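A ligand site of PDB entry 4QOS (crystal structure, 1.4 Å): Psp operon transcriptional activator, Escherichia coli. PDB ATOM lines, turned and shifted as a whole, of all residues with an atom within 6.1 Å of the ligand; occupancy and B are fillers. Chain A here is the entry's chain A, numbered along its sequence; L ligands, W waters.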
ATOM      1  N   LEU A   8     -10.039 -14.758  -8.028  1.00  0.00           N
ATOM      2  CA  LEU A   8      -9.106 -14.024  -8.873  1.00  0.00           C
ATOM      3  C   LEU A   8      -7.704 -13.981  -8.266  1.00  0.00           C
ATOM      4  O   LEU A   8      -6.859 -13.200  -8.699  1.00  0.00           O
ATOM      5  CB  LEU A   8      -9.620 -12.604  -9.113  1.00  0.00           C
ATOM      6  N   LEU A   9      -7.464 -14.826  -7.270  1.00  0.00           N
ATOM      7  CA  LEU A   9      -6.209 -14.786  -6.521  1.00  0.00           C
ATOM      8  C   LEU A   9      -5.062 -15.424  -7.283  1.00  0.00           C
ATOM      9  O   LEU A   9      -5.236 -16.425  -7.979  1.00  0.00           O
ATOM     10  CB  LEU A   9      -6.373 -15.497  -5.185  1.00  0.00           C
ATOM     11  CG  LEU A   9      -7.089 -14.759  -4.054  1.00  0.00           C
ATOM     12  CD1 LEU A   9      -8.350 -14.037  -4.525  1.00  0.00           C
ATOM     13  CD2 LEU A   9      -7.434 -15.762  -2.979  1.00  0.00           C
ATOM     14  N   GLY A  10      -3.874 -14.844  -7.143  1.00  0.00           N
ATOM     15  CA  GLY A  10      -2.681 -15.386  -7.760  1.00  0.00           C
ATOM     16  C   GLY A  10      -1.819 -14.300  -8.323  1.00  0.00           C
ATOM     17  O   GLY A  10      -2.298 -13.281  -8.826  1.00  0.00           O
ATOM     18  N   PHE A  15       0.055 -18.168 -13.870  1.00  0.00           N
ATOM     19  CA  PHE A  15      -1.346 -17.789 -13.784  1.00  0.00           C
ATOM     20  C   PHE A  15      -1.656 -16.468 -14.487  1.00  0.00           C
ATOM     21  O   PHE A  15      -2.654 -16.343 -15.192  1.00  0.00           O
ATOM     22  CB  PHE A  15      -1.774 -17.762 -12.304  1.00  0.00           C
ATOM     23  CG  PHE A  15      -3.184 -17.359 -12.114  1.00  0.00           C
ATOM     24  CD1 PHE A  15      -4.216 -18.190 -12.485  1.00  0.00           C
ATOM     25  CD2 PHE A  15      -3.477 -16.137 -11.550  1.00  0.00           C
ATOM     26  CE1 PHE A  15      -5.541 -17.799 -12.302  1.00  0.00           C
ATOM     27  CE2 PHE A  15      -4.788 -15.743 -11.357  1.00  0.00           C
ATOM     28  CZ  PHE A  15      -5.820 -16.574 -11.738  1.00  0.00           C
ATOM     29  N   GLY A  36      -6.578 -28.781 -17.300  1.00  0.00           N
ATOM     30  CA  GLY A  36      -6.156 -28.584 -15.938  1.00  0.00           C
ATOM     31  C   GLY A  36      -6.783 -29.573 -14.992  1.00  0.00           C
ATOM     32  O   GLY A  36      -7.826 -30.172 -15.285  1.00  0.00           O
ATOM     33  N   GLU A  37      -6.129 -29.761 -13.866  1.00  0.00           N
ATOM     34  CA  GLU A  37      -6.599 -30.635 -12.812  1.00  0.00           C
ATOM     35  C   GLU A  37      -7.861 -30.126 -12.133  1.00  0.00           C
ATOM     36  O   GLU A  37      -8.259 -28.969 -12.290  1.00  0.00           O
ATOM     37  CB  GLU A  37      -5.498 -30.829 -11.769  1.00  0.00           C
ATOM     38  CG  GLU A  37      -4.301 -31.582 -12.322  1.00  0.00           C
ATOM     39  CD  GLU A  37      -3.149 -31.710 -11.357  1.00  0.00           C
ATOM     40  OE1 GLU A  37      -3.347 -31.504 -10.151  1.00  0.00           O
ATOM     41  OE2 GLU A  37      -2.023 -32.015 -11.801  1.00  0.00           O
ATOM     42  N   ARG A  38      -8.518 -30.988 -11.366  1.00  0.00           N
ATOM     43  CA  ARG A  38      -9.665 -30.557 -10.610  1.00  0.00           C
ATOM     44  C   ARG A  38      -9.273 -29.423  -9.658  1.00  0.00           C
ATOM     45  O   ARG A  38      -8.177 -29.425  -9.092  1.00  0.00           O
ATOM     46  CB  ARG A  38     -10.281 -31.709  -9.788  1.00  0.00           C
ATOM     47  CG  ARG A  38      -9.493 -32.202  -8.614  1.00  0.00           C
ATOM     48  CD  ARG A  38     -10.343 -33.211  -7.814  1.00  0.00           C
ATOM     49  NE  ARG A  38      -9.677 -33.626  -6.586  1.00  0.00           N
ATOM     50  CZ  ARG A  38      -8.765 -34.563  -6.519  1.00  0.00           C
ATOM     51  NH1 ARG A  38      -8.438 -35.269  -7.590  1.00  0.00           N
ATOM     52  NH2 ARG A  38      -8.215 -34.842  -5.352  1.00  0.00           N
ATOM     53  N   GLY A  39     -10.167 -28.459  -9.483  1.00  0.00           N
ATOM     54  CA  GLY A  39      -9.962 -27.416  -8.515  1.00  0.00           C
ATOM     55  C   GLY A  39      -8.980 -26.344  -8.957  1.00  0.00           C
ATOM     56  O   GLY A  39      -8.558 -25.543  -8.133  1.00  0.00           O
ATOM     57  N   THR A  40      -8.650 -26.255 -10.250  1.00  0.00           N
ATOM     58  CA  THR A  40      -7.683 -25.265 -10.727  1.00  0.00           C
ATOM     59  C   THR A  40      -8.331 -24.024 -11.282  1.00  0.00           C
ATOM     60  O   THR A  40      -7.611 -23.083 -11.665  1.00  0.00           O
ATOM     61  CB  THR A  40      -6.726 -25.832 -11.792  1.00  0.00           C
ATOM     62  OG1 THR A  40      -7.495 -26.418 -12.877  1.00  0.00           O
ATOM     63  CG2 THR A  40      -5.808 -26.824 -11.197  1.00  0.00           C
ATOM     64  N   GLY A  41      -9.658 -24.002 -11.338  1.00  0.00           N
ATOM     65  CA  GLY A  41     -10.396 -22.840 -11.782  1.00  0.00           C
ATOM     66  C   GLY A  41     -10.913 -22.902 -13.218  1.00  0.00           C
ATOM     67  O   GLY A  41     -11.157 -21.873 -13.828  1.00  0.00           O
ATOM     68  N   LYS A  42     -11.099 -24.096 -13.776  1.00  0.00           N
ATOM     69  CA  LYS A  42     -11.485 -24.198 -15.184  1.00  0.00           C
ATOM     70  C   LYS A  42     -12.833 -23.559 -15.504  1.00  0.00           C
ATOM     71  O   LYS A  42     -12.972 -22.805 -16.483  1.00  0.00           O
ATOM     72  CB  LYS A  42     -11.427 -25.659 -15.629  1.00  0.00           C
ATOM     73  CG  LYS A  42     -10.015 -26.223 -15.519  1.00  0.00           C
ATOM     74  CD  LYS A  42      -9.822 -27.556 -16.215  1.00  0.00           C
ATOM     75  CE  LYS A  42     -10.773 -28.590 -15.683  1.00  0.00           C
ATOM     76  NZ  LYS A  42     -10.512 -28.844 -14.242  1.00  0.00           N
ATOM     77  N   GLU A  43     -13.838 -23.816 -14.688  1.00  0.00           N
ATOM     78  CA  GLU A  43     -15.124 -23.203 -14.943  1.00  0.00           C
ATOM     79  C   GLU A  43     -15.092 -21.682 -14.712  1.00  0.00           C
ATOM     80  O   GLU A  43     -15.769 -20.957 -15.424  1.00  0.00           O
ATOM     81  CB  GLU A  43     -16.261 -23.846 -14.117  1.00  0.00           C
ATOM     82  CG  GLU A  43     -17.626 -23.287 -14.502  1.00  0.00           C
ATOM     83  CD  GLU A  43     -18.811 -24.216 -14.216  1.00  0.00           C
ATOM     84  OE1 GLU A  43     -18.601 -25.359 -13.753  1.00  0.00           O
ATOM     85  OE2 GLU A  43     -19.962 -23.792 -14.485  1.00  0.00           O
ATOM     86  N   LEU A  44     -14.272 -21.222 -13.770  1.00  0.00           N
ATOM     87  CA  LEU A  44     -14.116 -19.780 -13.573  1.00  0.00           C
ATOM     88  C   LEU A  44     -13.508 -19.136 -14.835  1.00  0.00           C
ATOM     89  O   LEU A  44     -13.930 -18.048 -15.267  1.00  0.00           O
ATOM     90  CB  LEU A  44     -13.254 -19.491 -12.346  1.00  0.00           C
ATOM     91  CG  LEU A  44     -13.912 -19.710 -10.979  1.00  0.00           C
ATOM     92  CD1 LEU A  44     -12.956 -19.309  -9.870  1.00  0.00           C
ATOM     93  CD2 LEU A  44     -15.221 -18.926 -10.848  1.00  0.00           C
ATOM     94  N   ILE A  45     -12.536 -19.807 -15.446  1.00  0.00           N
ATOM     95  CA  ILE A  45     -11.914 -19.309 -16.669  1.00  0.00           C
ATOM     96  C   ILE A  45     -12.912 -19.341 -17.827  1.00  0.00           C
ATOM     97  O   ILE A  45     -12.943 -18.424 -18.651  1.00  0.00           O
ATOM     98  CB  ILE A  45     -10.667 -20.145 -16.990  1.00  0.00           C
ATOM     99  CG1 ILE A  45      -9.572 -19.933 -15.956  1.00  0.00           C
ATOM    100  CG2 ILE A  45     -10.160 -19.841 -18.381  1.00  0.00           C
ATOM    101  CD1 ILE A  45      -9.023 -18.514 -15.839  1.00  0.00           C
ATOM    102  N   PHE A 105     -20.241 -24.341 -21.845  1.00  0.00           N
ATOM    103  CA  PHE A 105     -19.065 -24.918 -21.207  1.00  0.00           C
ATOM    104  C   PHE A 105     -19.282 -26.409 -20.991  1.00  0.00           C
ATOM    105  O   PHE A 105     -20.186 -26.800 -20.252  1.00  0.00           O
ATOM    106  CB  PHE A 105     -18.740 -24.229 -19.871  1.00  0.00           C
ATOM    107  CG  PHE A 105     -17.627 -24.867 -19.093  1.00  0.00           C
ATOM    108  CD1 PHE A 105     -16.353 -25.011 -19.626  1.00  0.00           C
ATOM    109  CD2 PHE A 105     -17.848 -25.340 -17.796  1.00  0.00           C
ATOM    110  CE1 PHE A 105     -15.355 -25.594 -18.905  1.00  0.00           C
ATOM    111  CE2 PHE A 105     -16.855 -25.931 -17.085  1.00  0.00           C
ATOM    112  CZ  PHE A 105     -15.594 -26.055 -17.626  1.00  0.00           C
ATOM    113  N   ASP A 107     -17.596 -29.607 -19.428  1.00  0.00           N
ATOM    114  CA  ASP A 107     -16.567 -30.088 -18.532  1.00  0.00           C
ATOM    115  C   ASP A 107     -16.388 -31.605 -18.647  1.00  0.00           C
ATOM    116  O   ASP A 107     -17.319 -32.308 -19.056  1.00  0.00           O
ATOM    117  CB  ASP A 107     -16.943 -29.687 -17.098  1.00  0.00           C
ATOM    118  CG  ASP A 107     -15.750 -29.630 -16.173  1.00  0.00           C
ATOM    119  OD1 ASP A 107     -14.579 -29.778 -16.578  1.00  0.00           O
ATOM    120  OD2 ASP A 107     -15.993 -29.422 -14.964  1.00  0.00           O
ATOM    121  N   LEU A 176      -4.052 -24.586 -17.387  1.00  0.00           N
ATOM    122  CA  LEU A 176      -4.077 -24.012 -16.045  1.00  0.00           C
ATOM    123  C   LEU A 176      -3.059 -24.714 -15.174  1.00  0.00           C
ATOM    124  O   LEU A 176      -3.086 -25.941 -15.073  1.00  0.00           O
ATOM    125  CB  LEU A 176      -5.449 -24.150 -15.396  1.00  0.00           C
ATOM    126  CG  LEU A 176      -6.604 -23.502 -16.100  1.00  0.00           C
ATOM    127  CD1 LEU A 176      -7.773 -23.547 -15.126  1.00  0.00           C
ATOM    128  CD2 LEU A 176      -6.319 -22.076 -16.517  1.00  0.00           C
ATOM    129  N   ARG A 182       2.473 -23.414  -8.753  1.00  0.00           N
ATOM    130  CA  ARG A 182       2.263 -22.011  -8.452  1.00  0.00           C
ATOM    131  C   ARG A 182       2.642 -21.851  -6.989  1.00  0.00           C
ATOM    132  O   ARG A 182       1.870 -21.286  -6.219  1.00  0.00           O
ATOM    133  CB  ARG A 182       0.778 -21.601  -8.558  1.00  0.00           C
ATOM    134  CG  ARG A 182       0.062 -21.970  -9.842  1.00  0.00           C
ATOM    135  CD  ARG A 182      -1.455 -21.744  -9.728  1.00  0.00           C
ATOM    136  NE  ARG A 182      -1.767 -20.381  -9.313  1.00  0.00           N
ATOM    137  CZ  ARG A 182      -2.980 -19.851  -9.328  1.00  0.00           C
ATOM    138  NH1 ARG A 182      -4.030 -20.556  -9.769  1.00  0.00           N
ATOM    139  NH2 ARG A 182      -3.148 -18.603  -8.912  1.00  0.00           N
ATOM    140  N   MET A 189      -2.977 -17.598  -1.078  1.00  0.00           N
ATOM    141  CA  MET A 189      -4.332 -18.079  -1.049  1.00  0.00           C
ATOM    142  C   MET A 189      -4.672 -18.660   0.339  1.00  0.00           C
ATOM    143  O   MET A 189      -5.758 -18.460   0.833  1.00  0.00           O
ATOM    144  CB  MET A 189      -4.571 -19.147  -2.097  1.00  0.00           C
ATOM    145  CG  MET A 189      -4.539 -18.656  -3.520  1.00  0.00           C
ATOM    146  SD  MET A 189      -4.882 -20.064  -4.636  1.00  0.00           S
ATOM    147  CE  MET A 189      -4.661 -19.284  -6.222  1.00  0.00           C
ATOM    148  N   PHE A 193      -7.825 -17.432   2.523  1.00  0.00           N
ATOM    149  CA  PHE A 193      -8.859 -18.349   2.970  1.00  0.00           C
ATOM    150  C   PHE A 193      -8.945 -18.400   4.511  1.00  0.00           C
ATOM    151  O   PHE A 193     -10.028 -18.503   5.102  1.00  0.00           O
ATOM    152  CB  PHE A 193      -8.659 -19.759   2.409  1.00  0.00           C
ATOM    153  CG  PHE A 193      -8.814 -19.861   0.914  1.00  0.00           C
ATOM    154  CD1 PHE A 193      -9.808 -19.178   0.251  1.00  0.00           C
ATOM    155  CD2 PHE A 193      -7.950 -20.639   0.172  1.00  0.00           C
ATOM    156  CE1 PHE A 193      -9.948 -19.291  -1.155  1.00  0.00           C
ATOM    157  CE2 PHE A 193      -8.092 -20.763  -1.194  1.00  0.00           C
ATOM    158  CZ  PHE A 193      -9.067 -20.069  -1.848  1.00  0.00           C
ATOM    159  N   ILE A 226      -7.145 -25.676  -5.639  1.00  0.00           N
ATOM    160  CA  ILE A 226      -7.626 -24.553  -4.827  1.00  0.00           C
ATOM    161  C   ILE A 226      -8.835 -24.938  -3.966  1.00  0.00           C
ATOM    162  O   ILE A 226      -8.971 -24.478  -2.837  1.00  0.00           O
ATOM    163  CB  ILE A 226      -7.923 -23.336  -5.711  1.00  0.00           C
ATOM    164  CG1 ILE A 226      -6.654 -22.964  -6.486  1.00  0.00           C
ATOM    165  CG2 ILE A 226      -8.464 -22.156  -4.901  1.00  0.00           C
ATOM    166  CD1 ILE A 226      -6.926 -22.059  -7.656  1.00  0.00           C
ATOM    167  N   ARG A 227      -9.725 -25.799  -4.460  1.00  0.00           N
ATOM    168  CA  ARG A 227     -10.886 -26.243  -3.698  1.00  0.00           C
ATOM    169  C   ARG A 227     -10.405 -26.958  -2.428  1.00  0.00           C
ATOM    170  O   ARG A 227     -10.920 -26.720  -1.328  1.00  0.00           O
ATOM    171  CB  ARG A 227     -11.765 -27.154  -4.568  1.00  0.00           C
ATOM    172  CG  ARG A 227     -12.926 -27.803  -3.811  1.00  0.00           C
ATOM    173  CD  ARG A 227     -13.731 -28.766  -4.690  1.00  0.00           C
ATOM    174  NE  ARG A 227     -14.467 -28.133  -5.777  1.00  0.00           N
ATOM    175  CZ  ARG A 227     -14.152 -28.195  -7.071  1.00  0.00           C
ATOM    176  NH1 ARG A 227     -13.078 -28.850  -7.477  1.00  0.00           N
ATOM    177  NH2 ARG A 227     -14.929 -27.592  -7.966  1.00  0.00           N
ATOM    178  N   LYS A 230      -8.726 -24.490   0.121  1.00  0.00           N
ATOM    179  CA  LYS A 230      -9.734 -23.746   0.870  1.00  0.00           C
ATOM    180  C   LYS A 230     -10.288 -24.600   2.012  1.00  0.00           C
ATOM    181  O   LYS A 230     -10.399 -24.142   3.160  1.00  0.00           O
ATOM    182  CB  LYS A 230     -10.863 -23.254  -0.049  1.00  0.00           C
ATOM    183  CG  LYS A 230     -11.898 -22.449   0.678  1.00  0.00           C
ATOM    184  CD  LYS A 230     -12.914 -21.870  -0.283  1.00  0.00           C
ATOM    185  CE  LYS A 230     -13.941 -21.012   0.457  1.00  0.00           C
ATOM    186  NZ  LYS A 230     -14.918 -21.868   1.206  1.00  0.00           N
HETATM  187  P1  LIG L   1     -12.370 -26.557 -11.598  1.00  0.00           P
HETATM  188  O1  LIG L   1     -12.678 -27.755 -10.761  1.00  0.00           O
HETATM  189  O2  LIG L   1     -13.491 -26.093 -12.510  1.00  0.00           O
HETATM  190  O3  LIG L   1     -11.072 -26.732 -12.276  1.00  0.00           O
HETATM  191  P2  LIG L   1     -13.302 -24.240 -10.163  1.00  0.00           P
HETATM  192  O4  LIG L   1     -14.555 -24.997  -9.800  1.00  0.00           O
HETATM  193  O5  LIG L   1     -13.400 -23.152 -11.201  1.00  0.00           O
HETATM  194  O6  LIG L   1     -12.178 -25.350 -10.527  1.00  0.00           O
HETATM  195  O7  LIG L   1     -12.674 -23.608  -8.814  1.00  0.00           O
HETATM  196  C1  LIG L   1     -12.456 -24.457  -7.686  1.00  0.00           C
HETATM  197  C2  LIG L   1     -12.489 -23.635  -6.416  1.00  0.00           C
HETATM  198  O8  LIG L   1     -11.300 -22.859  -6.311  1.00  0.00           O
HETATM  199  C3  LIG L   1     -13.649 -22.643  -6.401  1.00  0.00           C
HETATM  200  O9  LIG L   1     -14.122 -22.483  -5.059  1.00  0.00           O
HETATM  201  C4  LIG L   1     -13.042 -21.349  -6.880  1.00  0.00           C
HETATM  202  O10 LIG L   1     -13.695 -20.189  -6.355  1.00  0.00           O
HETATM  203  C5  LIG L   1     -11.626 -21.472  -6.356  1.00  0.00           C
HETATM  204  N1  LIG L   1     -10.674 -20.781  -7.236  1.00  0.00           N
HETATM  205  C6  LIG L   1     -10.248 -21.218  -8.445  1.00  0.00           C
HETATM  206  N2  LIG L   1      -9.355 -20.335  -8.955  1.00  0.00           N
HETATM  207  C7  LIG L   1      -9.207 -19.337  -8.066  1.00  0.00           C
HETATM  208  C8  LIG L   1      -8.409 -18.101  -7.990  1.00  0.00           C
HETATM  209  N3  LIG L   1      -7.596 -17.774  -9.018  1.00  0.00           N
HETATM  210  N4  LIG L   1      -8.546 -17.329  -6.888  1.00  0.00           N
HETATM  211  C9  LIG L   1      -9.357 -17.668  -5.880  1.00  0.00           C
HETATM  212  N5  LIG L   1     -10.091 -18.782  -5.882  1.00  0.00           N
HETATM  213  C10 LIG L   1     -10.074 -19.637  -6.932  1.00  0.00           C
HETATM  214  O   HOH W   1     -16.370 -26.236 -11.242  1.00  0.00           O
HETATM  215  O   HOH W   2      -7.153 -20.460 -10.738  1.00  0.00           O
HETATM  216  O   HOH W   3     -16.690 -24.012  -8.088  1.00  0.00           O
HETATM  217  O   HOH W   4     -12.174 -18.457  -3.830  1.00  0.00           O
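Phe 15 touches the ligand.
O of Glu 37 touches O3 of the ligand, at 3.6 Å.
C of Arg 38 touches O1 of the ligand, at 3.9 Å.
Ile 226 touches the ligand (CG2 to O8, 3.2 Å).
13 residues have an atom within 4 Å of the ligand: Leu 8, Leu 9, Phe 15, Glu 37, Arg 38, Gly 39, Thr 40, Gly 41, Lys 42, Glu 43, Leu 44, Ile 226 and Arg 227.
The guanidinium group (NH2) of Arg 182 is in hydrogen-bond range of the backbone carbonyl oxygen (O) of Leu 9, at 3.2 Å.
O of Gly 39 is in hydrogen-bond range of N of Ile 226, 2.9 Å away.
The side-chain hydroxyl (OG1) of Thr 40 is in hydrogen-bond range of the backbone carbonyl oxygen (O) of Glu 37 (2.7 Å).
The side-chain amino group (NZ) of Lys 42 is in hydrogen-bond range of the backbone carbonyl oxygen (O) of Glu 37 (3.0 Å).
NZ of Lys 42 lies within hydrogen-bond range of O of Gly 36 (3.2 Å).
Water W1 lies within hydrogen-bond range of an oxygen (O4) of the ligand and the side-chain carboxylate (OE1) of Glu 43.
Water W2 lies within hydrogen-bond range of O of Thr 40 (2.8 Å), N2 of the ligand (2.8 Å) and NH1 of Arg 182 (3.3 Å).
N of Leu 9 is in hydrogen-bond range of N4 of the ligand, at 2.8 Å.
N of Glu 43 lies within hydrogen-bond range of O2 of the ligand, at 3.2 Å.
The backbone NH (N) of Leu 44 is in hydrogen-bond range of an oxygen (O5) of the ligand (3.3 Å).
N of Thr 40 is in hydrogen-bond range of O3 of the ligand.
The backbone carbonyl oxygen of Leu 9 sits at hydrogen-bond distance from a nitrogen (N3) of the ligand (2.9 Å).
An oxygen (O3) of the ligand lies within hydrogen-bond range of the backbone NH of Lys 42.
NZ of Lys 42 lies within salt-bridge range of O3 of the ligand, at 2.9 Å.
An oxygen (O6) of the ligand is in hydrogen-bond range of the backbone NH (N) of Gly 41.
N of Gly 39 lies within hydrogen-bond range of O1 of the ligand.
O4 of the ligand lies within salt-bridge range of NH2 of Arg 227, at 3.2 Å.
The backbone NH of Leu 8 lies within hydrogen-bond range of a nitrogen (N4) of the ligand (3.2 Å).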
